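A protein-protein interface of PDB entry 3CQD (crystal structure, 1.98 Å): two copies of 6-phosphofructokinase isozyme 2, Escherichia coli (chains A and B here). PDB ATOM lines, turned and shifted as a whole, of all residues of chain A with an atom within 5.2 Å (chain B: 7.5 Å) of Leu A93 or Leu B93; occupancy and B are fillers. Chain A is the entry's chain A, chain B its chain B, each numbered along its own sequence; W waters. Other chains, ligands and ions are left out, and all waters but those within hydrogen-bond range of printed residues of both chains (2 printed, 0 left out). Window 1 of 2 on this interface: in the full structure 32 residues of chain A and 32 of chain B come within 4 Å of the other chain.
OE1 of Gln A91 lies close to OE1 of Gln B91 (2.7 Å). The backbone carbonyl oxygen of Arg A105 sits at hydrogen-bond distance from the backbone NH of Leu B28, at 2.8 Å.
The backbone NH (N) of Thr A17 sits at hydrogen-bond distance from the backbone carbonyl oxygen (O) of His A94, 2.8 Å away. N of Met A108 is in hydrogen-bond range of OD1 of Asn A92 (2.7 Å). The backbone carbonyl oxygen (O) of Leu A93 is in hydrogen-bond range of the backbone NH (N) of Phe A106 (2.7 Å). OG1 of Thr B17 is in hydrogen-bond range of O of Thr B31 (2.5 Å). The backbone carbonyl oxygen (O) of Ile B18 is in hydrogen-bond range of the backbone NH (N) of Thr B31 (2.9 Å). The side-chain amide oxygen (OD1) of Asn B92 sits at hydrogen-bond distance from the backbone NH (N) of Met B108 (2.7 Å).
Hydrophobic or aromatic side chains of chain B that line the printed part of chain A: Leu B28, Pro B33, Leu B93, Val B95, Phe B106 and Met B108. Printed residues of chain A that touch a printed residue of chain B: Thr A17, Gln A91, Leu A93, Val A95, Arg A105, Phe A106 and Met A108. Hydrophobic or aromatic side chains of chain A that line the printed part of chain B: Leu A93, Val A95, Phe A106 and Met A108. Along chain A the printed residues that touch a printed residue of chain B span positions 17 to 108. Among the printed residues, no Asp or Glu carboxylate lies within 4 Å of a Lys or Arg side-chain nitrogen of the other chain.
Leu A93 touches three residues of chain B. Tyr A104 touches none of the printed residues of chain B. Of the printed residues of chain B, Arg A105 touches Leu B28 (2.8 Å). Of the printed residues of chain B, Met A108 touches Thr B17 (3.7 Å), Cys B30 (3.6 Å), Thr B31 (3.6 Å), Pro B33 (3.99 Å) and Leu B93 (3.7 Å). Printed residues of chain A within 4 Å of Cys B30: Phe A106 (3.96 Å) and Met A108 (3.6 Å). Of the printed residues of chain A, Leu B93 touches Leu A93 (3.6 Å), Phe A106 (3.6 Å) and Met A108 (3.7 Å). Val B107 touches none of the printed residues of chain A. The nearest residue of chain B that does not touch Leu A93 is Gln B91 (6.1 Å). The nearest printed residue of chain A that does not touch Leu B93 is Asn A92 (6.2 Å).
Thr A17 touches Met B108, and with the chains exchanged Met A108 touches Thr B17. Leu B93 touches its own counterpart, Leu A93. Leu A93 touches Phe B106, and with the chains exchanged Phe A106 touches Leu B93. Leu A93 touches Met B108, and with the chains exchanged Met A108 touches Leu B93. Of the 17 pairs that touch across the chains among the printed residues, 11 have their exchanged pair printed and touching as well.
Water W2 bridges OE1 of Gln B91 and N of Gln A91. Water W1 lies within hydrogen-bond range of the backbone NH (N) of Gln B91 and the side-chain amide nitrogen (NE2) of Gln A91.
Among the printed residues, merely in contact across the chains: Thr A17 with Met B108, Leu A93 with Leu B93, Leu A93 with Phe B106, Leu A93 with Met B108, Val A95 with Phe B106, Phe A106 with Leu B28, Phe A106 with Cys B30, Phe A106 with Leu B93, Phe A106 with Val B95, Phe A106 with Phe B106, Met A108 with Thr B17, Met A108 with Cys B30, Met A108 with Thr B31, Met A108 with Pro B33 and Met A108 with Leu B93.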
ATOM      1  N   ASP A  14     -21.809   7.517  15.701  1.00  0.00           N
ATOM      2  CA  ASP A  14     -21.503   6.797  14.474  1.00  0.00           C
ATOM      3  C   ASP A  14     -22.056   5.378  14.489  1.00  0.00           C
ATOM      4  O   ASP A  14     -22.101   4.727  15.531  1.00  0.00           O
ATOM      5  CB  ASP A  14     -20.011   6.845  14.162  1.00  0.00           C
ATOM      6  CG  ASP A  14     -19.511   8.265  13.993  1.00  0.00           C
ATOM      7  OD1 ASP A  14     -20.332   9.154  13.664  1.00  0.00           O
ATOM      8  OD2 ASP A  14     -18.312   8.500  14.228  1.00  0.00           O
ATOM      9  N   SER A  15     -22.540   4.958  13.333  1.00  0.00           N
ATOM     10  CA  SER A  15     -23.041   3.615  13.127  1.00  0.00           C
ATOM     11  C   SER A  15     -21.940   2.783  12.474  1.00  0.00           C
ATOM     12  O   SER A  15     -21.440   3.150  11.412  1.00  0.00           O
ATOM     13  CB  SER A  15     -24.261   3.674  12.219  1.00  0.00           C
ATOM     14  OG  SER A  15     -25.388   4.149  12.912  1.00  0.00           O
ATOM     15  N   THR A  17     -21.327  -0.744  10.819  1.00  0.00           N
ATOM     16  CA  THR A  17     -22.150  -1.775  10.223  1.00  0.00           C
ATOM     17  C   THR A  17     -21.314  -2.647   9.293  1.00  0.00           C
ATOM     18  O   THR A  17     -20.235  -2.265   8.839  1.00  0.00           O
ATOM     19  CB  THR A  17     -23.376  -1.160   9.471  1.00  0.00           C
ATOM     20  OG1 THR A  17     -24.270  -2.200   9.049  1.00  0.00           O
ATOM     21  CG2 THR A  17     -22.949  -0.351   8.240  1.00  0.00           C
ATOM     22  N   GLN A  91     -25.132  11.347  12.635  1.00  0.00           N
ATOM     23  CA  GLN A  91     -24.588  10.015  12.609  1.00  0.00           C
ATOM     24  C   GLN A  91     -23.745   9.822  11.379  1.00  0.00           C
ATOM     25  O   GLN A  91     -24.213  10.029  10.261  1.00  0.00           O
ATOM     26  CB  GLN A  91     -25.732   9.009  12.609  1.00  0.00           C
ATOM     27  CG  GLN A  91     -26.709   9.248  13.752  1.00  0.00           C
ATOM     28  CD  GLN A  91     -27.923   8.357  13.674  1.00  0.00           C
ATOM     29  OE1 GLN A  91     -28.994   8.786  13.229  1.00  0.00           O
ATOM     30  NE2 GLN A  91     -27.773   7.115  14.116  1.00  0.00           N
ATOM     31  N   ASN A  92     -22.490   9.454  11.587  1.00  0.00           N
ATOM     32  CA  ASN A  92     -21.663   9.039  10.470  1.00  0.00           C
ATOM     33  C   ASN A  92     -21.765   7.533  10.326  1.00  0.00           C
ATOM     34  O   ASN A  92     -22.245   6.835  11.234  1.00  0.00           O
ATOM     35  CB  ASN A  92     -20.222   9.543  10.627  1.00  0.00           C
ATOM     36  CG  ASN A  92     -20.136  11.048  10.496  1.00  0.00           C
ATOM     37  OD1 ASN A  92     -20.950  11.657   9.812  1.00  0.00           O
ATOM     38  ND2 ASN A  92     -19.176  11.649  11.156  1.00  0.00           N
ATOM     39  N   LEU A  93     -21.351   7.033   9.171  1.00  0.00           N
ATOM     40  CA  LEU A  93     -21.530   5.632   8.887  1.00  0.00           C
ATOM     41  C   LEU A  93     -20.201   5.007   8.564  1.00  0.00           C
ATOM     42  O   LEU A  93     -19.489   5.474   7.670  1.00  0.00           O
ATOM     43  CB  LEU A  93     -22.509   5.420   7.720  1.00  0.00           C
ATOM     44  CG  LEU A  93     -22.856   3.952   7.468  1.00  0.00           C
ATOM     45  CD1 LEU A  93     -23.614   3.357   8.647  1.00  0.00           C
ATOM     46  CD2 LEU A  93     -23.667   3.778   6.178  1.00  0.00           C
ATOM     47  N   HIS A  94     -19.891   3.941   9.294  1.00  0.00           N
ATOM     48  CA  HIS A  94     -18.698   3.146   9.083  1.00  0.00           C
ATOM     49  C   HIS A  94     -19.146   1.791   8.613  1.00  0.00           C
ATOM     50  O   HIS A  94     -19.820   1.066   9.342  1.00  0.00           O
ATOM     51  CB  HIS A  94     -17.889   3.033  10.384  1.00  0.00           C
ATOM     52  CG  HIS A  94     -17.211   4.305  10.781  1.00  0.00           C
ATOM     53  ND1 HIS A  94     -16.079   4.331  11.571  1.00  0.00           N
ATOM     54  CD2 HIS A  94     -17.488   5.598  10.476  1.00  0.00           C
ATOM     55  CE1 HIS A  94     -15.698   5.587  11.747  1.00  0.00           C
ATOM     56  NE2 HIS A  94     -16.535   6.372  11.087  1.00  0.00           N
ATOM     57  N   VAL A  95     -18.811   1.466   7.372  1.00  0.00           N
ATOM     58  CA  VAL A  95     -19.240   0.208   6.788  1.00  0.00           C
ATOM     59  C   VAL A  95     -18.036  -0.696   6.642  1.00  0.00           C
ATOM     60  O   VAL A  95     -17.073  -0.327   5.973  1.00  0.00           O
ATOM     61  CB  VAL A  95     -19.866   0.401   5.376  1.00  0.00           C
ATOM     62  CG1 VAL A  95     -20.365  -0.934   4.819  1.00  0.00           C
ATOM     63  CG2 VAL A  95     -20.977   1.421   5.399  1.00  0.00           C
ATOM     64  N   TYR A 104     -15.310   1.525   5.056  1.00  0.00           N
ATOM     65  CA  TYR A 104     -15.672   2.747   4.387  1.00  0.00           C
ATOM     66  C   TYR A 104     -16.225   3.676   5.447  1.00  0.00           C
ATOM     67  O   TYR A 104     -16.967   3.258   6.338  1.00  0.00           O
ATOM     68  CB  TYR A 104     -16.698   2.479   3.282  1.00  0.00           C
ATOM     69  CG  TYR A 104     -16.096   1.777   2.084  1.00  0.00           C
ATOM     70  CD1 TYR A 104     -15.870   0.406   2.099  1.00  0.00           C
ATOM     71  CD2 TYR A 104     -15.727   2.493   0.949  1.00  0.00           C
ATOM     72  CE1 TYR A 104     -15.311  -0.237   1.002  1.00  0.00           C
ATOM     73  CE2 TYR A 104     -15.154   1.867  -0.138  1.00  0.00           C
ATOM     74  CZ  TYR A 104     -14.952   0.496  -0.104  1.00  0.00           C
ATOM     75  OH  TYR A 104     -14.387  -0.121  -1.184  1.00  0.00           O
ATOM     76  N   ARG A 105     -15.845   4.936   5.362  1.00  0.00           N
ATOM     77  CA  ARG A 105     -16.212   5.877   6.395  1.00  0.00           C
ATOM     78  C   ARG A 105     -16.874   7.038   5.734  1.00  0.00           C
ATOM     79  O   ARG A 105     -16.208   7.812   5.035  1.00  0.00           O
ATOM     80  CB  ARG A 105     -14.968   6.359   7.131  1.00  0.00           C
ATOM     81  CG  ARG A 105     -14.198   5.235   7.762  1.00  0.00           C
ATOM     82  CD  ARG A 105     -12.745   5.605   7.771  1.00  0.00           C
ATOM     83  NE  ARG A 105     -12.464   6.463   8.896  1.00  0.00           N
ATOM     84  CZ  ARG A 105     -11.322   7.120   9.095  1.00  0.00           C
ATOM     85  NH1 ARG A 105     -10.308   7.048   8.238  1.00  0.00           N
ATOM     86  NH2 ARG A 105     -11.201   7.842  10.184  1.00  0.00           N
ATOM     87  N   PHE A 106     -18.177   7.151   5.951  1.00  0.00           N
ATOM     88  CA  PHE A 106     -18.952   8.247   5.405  1.00  0.00           C
ATOM     89  C   PHE A 106     -19.153   9.308   6.464  1.00  0.00           C
ATOM     90  O   PHE A 106     -19.835   9.107   7.465  1.00  0.00           O
ATOM     91  CB  PHE A 106     -20.263   7.733   4.808  1.00  0.00           C
ATOM     92  CG  PHE A 106     -20.041   6.711   3.744  1.00  0.00           C
ATOM     93  CD1 PHE A 106     -20.056   5.355   4.057  1.00  0.00           C
ATOM     94  CD2 PHE A 106     -19.744   7.099   2.446  1.00  0.00           C
ATOM     95  CE1 PHE A 106     -19.805   4.395   3.085  1.00  0.00           C
ATOM     96  CE2 PHE A 106     -19.490   6.148   1.466  1.00  0.00           C
ATOM     97  CZ  PHE A 106     -19.516   4.789   1.790  1.00  0.00           C
ATOM     98  N   MET A 108     -20.274  12.846   7.450  1.00  0.00           N
ATOM     99  CA  MET A 108     -21.134  14.007   7.226  1.00  0.00           C
ATOM    100  C   MET A 108     -20.893  15.054   8.297  1.00  0.00           C
ATOM    101  O   MET A 108     -20.265  14.758   9.309  1.00  0.00           O
ATOM    102  CB  MET A 108     -22.605  13.580   7.210  1.00  0.00           C
ATOM    103  CG  MET A 108     -22.981  12.950   5.879  1.00  0.00           C
ATOM    104  SD  MET A 108     -24.497  12.000   5.894  1.00  0.00           S
ATOM    105  CE  MET A 108     -23.956  10.653   6.953  1.00  0.00           C
ATOM    106  N   SER B  12     -37.693   4.635   8.000  1.00  0.00           N
ATOM    107  CA  SER B  12     -36.418   5.243   8.245  1.00  0.00           C
ATOM    108  C   SER B  12     -36.459   6.667   7.788  1.00  0.00           C
ATOM    109  O   SER B  12     -37.340   7.077   7.016  1.00  0.00           O
ATOM    110  CB  SER B  12     -35.274   4.473   7.541  1.00  0.00           C
ATOM    111  OG  SER B  12     -35.476   4.376   6.148  1.00  0.00           O
ATOM    112  N   LEU B  13     -35.525   7.442   8.308  1.00  0.00           N
ATOM    113  CA  LEU B  13     -35.309   8.760   7.787  1.00  0.00           C
ATOM    114  C   LEU B  13     -33.949   8.685   7.141  1.00  0.00           C
ATOM    115  O   LEU B  13     -32.953   8.670   7.819  1.00  0.00           O
ATOM    116  CB  LEU B  13     -35.344   9.818   8.892  1.00  0.00           C
ATOM    117  CG  LEU B  13     -35.100  11.236   8.375  1.00  0.00           C
ATOM    118  CD1 LEU B  13     -36.362  11.780   7.699  1.00  0.00           C
ATOM    119  CD2 LEU B  13     -34.642  12.127   9.516  1.00  0.00           C
ATOM    120  N   ASP B  14     -33.930   8.617   5.819  1.00  0.00           N
ATOM    121  CA  ASP B  14     -32.689   8.406   5.103  1.00  0.00           C
ATOM    122  C   ASP B  14     -31.942   9.673   4.824  1.00  0.00           C
ATOM    123  O   ASP B  14     -32.531  10.720   4.534  1.00  0.00           O
ATOM    124  CB  ASP B  14     -32.939   7.603   3.825  1.00  0.00           C
ATOM    125  CG  ASP B  14     -33.618   6.284   4.123  1.00  0.00           C
ATOM    126  OD1 ASP B  14     -33.504   5.821   5.280  1.00  0.00           O
ATOM    127  OD2 ASP B  14     -34.273   5.720   3.235  1.00  0.00           O
ATOM    128  N   SER B  15     -30.627   9.561   4.940  1.00  0.00           N
ATOM    129  CA  SER B  15     -29.735  10.640   4.607  1.00  0.00           C
ATOM    130  C   SER B  15     -29.216  10.425   3.188  1.00  0.00           C
ATOM    131  O   SER B  15     -28.609   9.400   2.886  1.00  0.00           O
ATOM    132  CB  SER B  15     -28.587  10.676   5.607  1.00  0.00           C
ATOM    133  OG  SER B  15     -29.030  11.147   6.867  1.00  0.00           O
ATOM    134  N   ALA B  16     -29.491  11.377   2.311  1.00  0.00           N
ATOM    135  CA  ALA B  16     -28.896  11.357   0.983  1.00  0.00           C
ATOM    136  C   ALA B  16     -27.748  12.346   1.001  1.00  0.00           C
ATOM    137  O   ALA B  16     -27.923  13.510   1.355  1.00  0.00           O
ATOM    138  CB  ALA B  16     -29.912  11.724  -0.073  1.00  0.00           C
ATOM    139  N   THR B  17     -26.569  11.870   0.640  1.00  0.00           N
ATOM    140  CA  THR B  17     -25.359  12.679   0.718  1.00  0.00           C
ATOM    141  C   THR B  17     -24.528  12.489  -0.548  1.00  0.00           C
ATOM    142  O   THR B  17     -24.726  11.539  -1.306  1.00  0.00           O
ATOM    143  CB  THR B  17     -24.543  12.361   2.014  1.00  0.00           C
ATOM    144  OG1 THR B  17     -23.494  13.321   2.199  1.00  0.00           O
ATOM    145  CG2 THR B  17     -23.967  10.936   1.995  1.00  0.00           C
ATOM    146  N   ILE B  18     -23.623  13.432  -0.778  1.00  0.00           N
ATOM    147  CA  ILE B  18     -22.787  13.428  -1.960  1.00  0.00           C
ATOM    148  C   ILE B  18     -21.354  13.457  -1.479  1.00  0.00           C
ATOM    149  O   ILE B  18     -21.034  14.110  -0.493  1.00  0.00           O
ATOM    150  CB  ILE B  18     -23.052  14.668  -2.821  1.00  0.00           C
ATOM    151  CG1 ILE B  18     -24.541  14.764  -3.184  1.00  0.00           C
ATOM    152  CG2 ILE B  18     -22.135  14.695  -4.081  1.00  0.00           C
ATOM    153  CD1 ILE B  18     -24.995  16.164  -3.501  1.00  0.00           C
ATOM    154  N   LEU B  28     -14.473   9.667   3.891  1.00  0.00           N
ATOM    155  CA  LEU B  28     -15.150  10.236   2.745  1.00  0.00           C
ATOM    156  C   LEU B  28     -15.978  11.388   3.253  1.00  0.00           C
ATOM    157  O   LEU B  28     -16.920  11.191   4.025  1.00  0.00           O
ATOM    158  CB  LEU B  28     -16.010   9.181   2.030  1.00  0.00           C
ATOM    159  CG  LEU B  28     -15.197   7.927   1.677  1.00  0.00           C
ATOM    160  CD1 LEU B  28     -16.088   6.808   1.163  1.00  0.00           C
ATOM    161  CD2 LEU B  28     -14.097   8.241   0.656  1.00  0.00           C
ATOM    162  N   CYS B  30     -18.658  13.819   3.211  1.00  0.00           N
ATOM    163  CA  CYS B  30     -19.977  13.788   2.606  1.00  0.00           C
ATOM    164  C   CYS B  30     -20.714  15.064   2.928  1.00  0.00           C
ATOM    165  O   CYS B  30     -20.578  15.616   4.023  1.00  0.00           O
ATOM    166  CB  CYS B  30     -20.772  12.589   3.119  1.00  0.00           C
ATOM    167  SG  CYS B  30     -20.114  11.033   2.632  1.00  0.00           S
ATOM    168  N   THR B  31     -21.478  15.542   1.960  1.00  0.00           N
ATOM    169  CA  THR B  31     -22.226  16.781   2.116  1.00  0.00           C
ATOM    170  C   THR B  31     -23.315  16.608   3.163  1.00  0.00           C
ATOM    171  O   THR B  31     -23.756  15.471   3.449  1.00  0.00           O
ATOM    172  CB  THR B  31     -22.876  17.198   0.788  1.00  0.00           C
ATOM    173  OG1 THR B  31     -23.750  16.150   0.352  1.00  0.00           O
ATOM    174  CG2 THR B  31     -21.816  17.469  -0.290  1.00  0.00           C
ATOM    175  N   PRO B  33     -26.552  16.020   4.660  1.00  0.00           N
ATOM    176  CA  PRO B  33     -27.543  15.168   4.034  1.00  0.00           C
ATOM    177  C   PRO B  33     -28.836  15.889   3.720  1.00  0.00           C
ATOM    178  O   PRO B  33     -29.219  16.845   4.408  1.00  0.00           O
ATOM    179  CB  PRO B  33     -27.797  14.088   5.095  1.00  0.00           C
ATOM    180  CG  PRO B  33     -27.462  14.748   6.387  1.00  0.00           C
ATOM    181  CD  PRO B  33     -26.271  15.603   6.046  1.00  0.00           C
ATOM    182  N   GLU B  36     -34.716  12.009   3.418  1.00  0.00           N
ATOM    183  CA  GLU B  36     -35.662  11.360   2.521  1.00  0.00           C
ATOM    184  C   GLU B  36     -36.476  10.401   3.379  1.00  0.00           C
ATOM    185  O   GLU B  36     -35.923   9.808   4.306  1.00  0.00           O
ATOM    186  CB  GLU B  36     -34.897  10.531   1.480  1.00  0.00           C
ATOM    187  CG  GLU B  36     -33.836  11.281   0.714  1.00  0.00           C
ATOM    188  CD  GLU B  36     -33.079  10.391  -0.246  1.00  0.00           C
ATOM    189  OE1 GLU B  36     -32.671   9.269   0.146  1.00  0.00           O
ATOM    190  OE2 GLU B  36     -32.868  10.821  -1.392  1.00  0.00           O
ATOM    191  N   GLN B  91     -31.804   5.571  10.465  1.00  0.00           N
ATOM    192  CA  GLN B  91     -31.358   6.226   9.255  1.00  0.00           C
ATOM    193  C   GLN B  91     -30.581   5.306   8.347  1.00  0.00           C
ATOM    194  O   GLN B  91     -29.593   4.680   8.751  1.00  0.00           O
ATOM    195  CB  GLN B  91     -30.532   7.457   9.610  1.00  0.00           C
ATOM    196  CG  GLN B  91     -31.364   8.461  10.433  1.00  0.00           C
ATOM    197  CD  GLN B  91     -30.810   9.855  10.406  1.00  0.00           C
ATOM    198  OE1 GLN B  91     -29.731  10.123  10.942  1.00  0.00           O
ATOM    199  NE2 GLN B  91     -31.544  10.765   9.782  1.00  0.00           N
ATOM    200  N   ASN B  92     -31.041   5.213   7.108  1.00  0.00           N
ATOM    201  CA  ASN B  92     -30.245   4.592   6.077  1.00  0.00           C
ATOM    202  C   ASN B  92     -29.467   5.681   5.361  1.00  0.00           C
ATOM    203  O   ASN B  92     -29.799   6.877   5.470  1.00  0.00           O
ATOM    204  CB  ASN B  92     -31.128   3.809   5.111  1.00  0.00           C
ATOM    205  CG  ASN B  92     -31.724   2.575   5.747  1.00  0.00           C
ATOM    206  OD1 ASN B  92     -31.157   1.993   6.673  1.00  0.00           O
ATOM    207  ND2 ASN B  92     -32.881   2.179   5.262  1.00  0.00           N
ATOM    208  N   LEU B  93     -28.407   5.280   4.672  1.00  0.00           N
ATOM    209  CA  LEU B  93     -27.565   6.229   3.983  1.00  0.00           C
ATOM    210  C   LEU B  93     -27.562   5.972   2.497  1.00  0.00           C
ATOM    211  O   LEU B  93     -27.309   4.849   2.037  1.00  0.00           O
ATOM    212  CB  LEU B  93     -26.135   6.189   4.533  1.00  0.00           C
ATOM    213  CG  LEU B  93     -25.181   7.254   3.987  1.00  0.00           C
ATOM    214  CD1 LEU B  93     -25.662   8.675   4.341  1.00  0.00           C
ATOM    215  CD2 LEU B  93     -23.765   7.008   4.508  1.00  0.00           C
ATOM    216  N   HIS B  94     -27.856   7.027   1.755  1.00  0.00           N
ATOM    217  CA  HIS B  94     -27.759   7.033   0.314  1.00  0.00           C
ATOM    218  C   HIS B  94     -26.612   7.962  -0.041  1.00  0.00           C
ATOM    219  O   HIS B  94     -26.631   9.134   0.312  1.00  0.00           O
ATOM    220  CB  HIS B  94     -29.073   7.510  -0.314  1.00  0.00           C
ATOM    221  CG  HIS B  94     -30.206   6.560  -0.114  1.00  0.00           C
ATOM    222  ND1 HIS B  94     -31.522   6.906  -0.341  1.00  0.00           N
ATOM    223  CD2 HIS B  94     -30.222   5.271   0.310  1.00  0.00           C
ATOM    224  CE1 HIS B  94     -32.296   5.866  -0.080  1.00  0.00           C
ATOM    225  NE2 HIS B  94     -31.530   4.862   0.320  1.00  0.00           N
ATOM    226  N   VAL B  95     -25.591   7.408  -0.675  1.00  0.00           N
ATOM    227  CA  VAL B  95     -24.394   8.146  -1.028  1.00  0.00           C
ATOM    228  C   VAL B  95     -24.252   8.245  -2.541  1.00  0.00           C
ATOM    229  O   VAL B  95     -24.144   7.225  -3.224  1.00  0.00           O
ATOM    230  CB  VAL B  95     -23.136   7.471  -0.437  1.00  0.00           C
ATOM    231  CG1 VAL B  95     -21.911   8.269  -0.773  1.00  0.00           C
ATOM    232  CG2 VAL B  95     -23.290   7.332   1.046  1.00  0.00           C
ATOM    233  N   HIS B  96     -24.246   9.476  -3.047  1.00  0.00           N
ATOM    234  CA  HIS B  96     -24.003   9.722  -4.447  1.00  0.00           C
ATOM    235  C   HIS B  96     -22.542  10.066  -4.576  1.00  0.00           C
ATOM    236  O   HIS B  96     -22.053  10.967  -3.897  1.00  0.00           O
ATOM    237  CB  HIS B  96     -24.828  10.885  -4.986  1.00  0.00           C
ATOM    238  CG  HIS B  96     -24.587  11.148  -6.440  1.00  0.00           C
ATOM    239  ND1 HIS B  96     -25.260  10.472  -7.438  1.00  0.00           N
ATOM    240  CD2 HIS B  96     -23.709  11.970  -7.067  1.00  0.00           C
ATOM    241  CE1 HIS B  96     -24.829  10.892  -8.616  1.00  0.00           C
ATOM    242  NE2 HIS B  96     -23.892  11.803  -8.419  1.00  0.00           N
ATOM    243  N   GLN B 103     -24.597   5.668  -7.115  1.00  0.00           N
ATOM    244  CA  GLN B 103     -25.252   5.853  -5.830  1.00  0.00           C
ATOM    245  C   GLN B 103     -25.120   4.565  -5.035  1.00  0.00           C
ATOM    246  O   GLN B 103     -25.208   3.446  -5.571  1.00  0.00           O
ATOM    247  CB  GLN B 103     -26.721   6.264  -6.005  1.00  0.00           C
ATOM    248  CG  GLN B 103     -27.504   5.298  -6.853  1.00  0.00           C
ATOM    249  CD  GLN B 103     -28.922   5.748  -7.188  1.00  0.00           C
ATOM    250  OE1 GLN B 103     -29.557   5.175  -8.078  1.00  0.00           O
ATOM    251  NE2 GLN B 103     -29.427   6.769  -6.479  1.00  0.00           N
ATOM    252  N   TYR B 104     -24.799   4.710  -3.789  1.00  0.00           N
ATOM    253  CA  TYR B 104     -24.678   3.603  -2.911  1.00  0.00           C
ATOM    254  C   TYR B 104     -25.800   3.662  -1.899  1.00  0.00           C
ATOM    255  O   TYR B 104     -26.149   4.689  -1.489  1.00  0.00           O
ATOM    256  CB  TYR B 104     -23.284   3.555  -2.302  1.00  0.00           C
ATOM    257  CG  TYR B 104     -22.196   3.286  -3.310  1.00  0.00           C
ATOM    258  CD1 TYR B 104     -21.678   4.272  -4.085  1.00  0.00           C
ATOM    259  CD2 TYR B 104     -21.694   2.032  -3.463  1.00  0.00           C
ATOM    260  CE1 TYR B 104     -20.710   4.003  -4.983  1.00  0.00           C
ATOM    261  CE2 TYR B 104     -20.768   1.764  -4.339  1.00  0.00           C
ATOM    262  CZ  TYR B 104     -20.250   2.737  -5.101  1.00  0.00           C
ATOM    263  OH  TYR B 104     -19.280   2.422  -5.956  1.00  0.00           O
ATOM    264  N   ARG B 105     -26.379   2.549  -1.557  1.00  0.00           N
ATOM    265  CA  ARG B 105     -27.408   2.544  -0.583  1.00  0.00           C
ATOM    266  C   ARG B 105     -27.105   1.581   0.506  1.00  0.00           C
ATOM    267  O   ARG B 105     -26.876   0.454   0.258  1.00  0.00           O
ATOM    268  CB  ARG B 105     -28.777   2.295  -1.191  1.00  0.00           C
ATOM    269  CG  ARG B 105     -29.152   3.132  -2.345  1.00  0.00           C
ATOM    270  CD  ARG B 105     -29.733   2.281  -3.431  1.00  0.00           C
ATOM    271  NE  ARG B 105     -31.100   2.070  -3.155  1.00  0.00           N
ATOM    272  CZ  ARG B 105     -31.938   1.288  -3.789  1.00  0.00           C
ATOM    273  NH1 ARG B 105     -31.629   0.555  -4.804  1.00  0.00           N
ATOM    274  NH2 ARG B 105     -33.134   1.281  -3.360  1.00  0.00           N
ATOM    275  N   PHE B 106     -27.013   2.115   1.697  1.00  0.00           N
ATOM    276  CA  PHE B 106     -26.707   1.392   2.887  1.00  0.00           C
ATOM    277  C   PHE B 106     -27.976   1.234   3.725  1.00  0.00           C
ATOM    278  O   PHE B 106     -28.450   2.171   4.318  1.00  0.00           O
ATOM    279  CB  PHE B 106     -25.530   1.998   3.665  1.00  0.00           C
ATOM    280  CG  PHE B 106     -24.278   2.148   2.852  1.00  0.00           C
ATOM    281  CD1 PHE B 106     -23.959   3.331   2.260  1.00  0.00           C
ATOM    282  CD2 PHE B 106     -23.462   1.080   2.620  1.00  0.00           C
ATOM    283  CE1 PHE B 106     -22.865   3.436   1.486  1.00  0.00           C
ATOM    284  CE2 PHE B 106     -22.364   1.219   1.843  1.00  0.00           C
ATOM    285  CZ  PHE B 106     -22.076   2.374   1.281  1.00  0.00           C
ATOM    286  N   VAL B 107     -28.498   0.025   3.732  1.00  0.00           N
ATOM    287  CA  VAL B 107     -29.782  -0.264   4.353  1.00  0.00           C
ATOM    288  C   VAL B 107     -29.548  -1.038   5.637  1.00  0.00           C
ATOM    289  O   VAL B 107     -29.035  -2.167   5.626  1.00  0.00           O
ATOM    290  CB  VAL B 107     -30.729  -1.025   3.380  1.00  0.00           C
ATOM    291  CG1 VAL B 107     -32.156  -1.139   3.975  1.00  0.00           C
ATOM    292  CG2 VAL B 107     -30.783  -0.303   2.057  1.00  0.00           C
ATOM    293  N   MET B 108     -29.892  -0.394   6.746  1.00  0.00           N
ATOM    294  CA  MET B 108     -29.840  -1.013   8.051  1.00  0.00           C
ATOM    295  C   MET B 108     -31.257  -1.243   8.545  1.00  0.00           C
ATOM    296  O   MET B 108     -32.201  -0.718   7.956  1.00  0.00           O
ATOM    297  CB  MET B 108     -29.060  -0.139   9.026  1.00  0.00           C
ATOM    298  CG  MET B 108     -27.582  -0.206   8.770  1.00  0.00           C
ATOM    299  SD  MET B 108     -26.705   1.172   9.467  1.00  0.00           S
ATOM    300  CE  MET B 108     -27.169   2.466   8.315  1.00  0.00           C
HETATM  301  O   HOH W   1     -29.545   5.222  12.463  1.00  0.00           O
HETATM  302  O   HOH W   2     -27.545  11.787  10.835  1.00  0.00           O
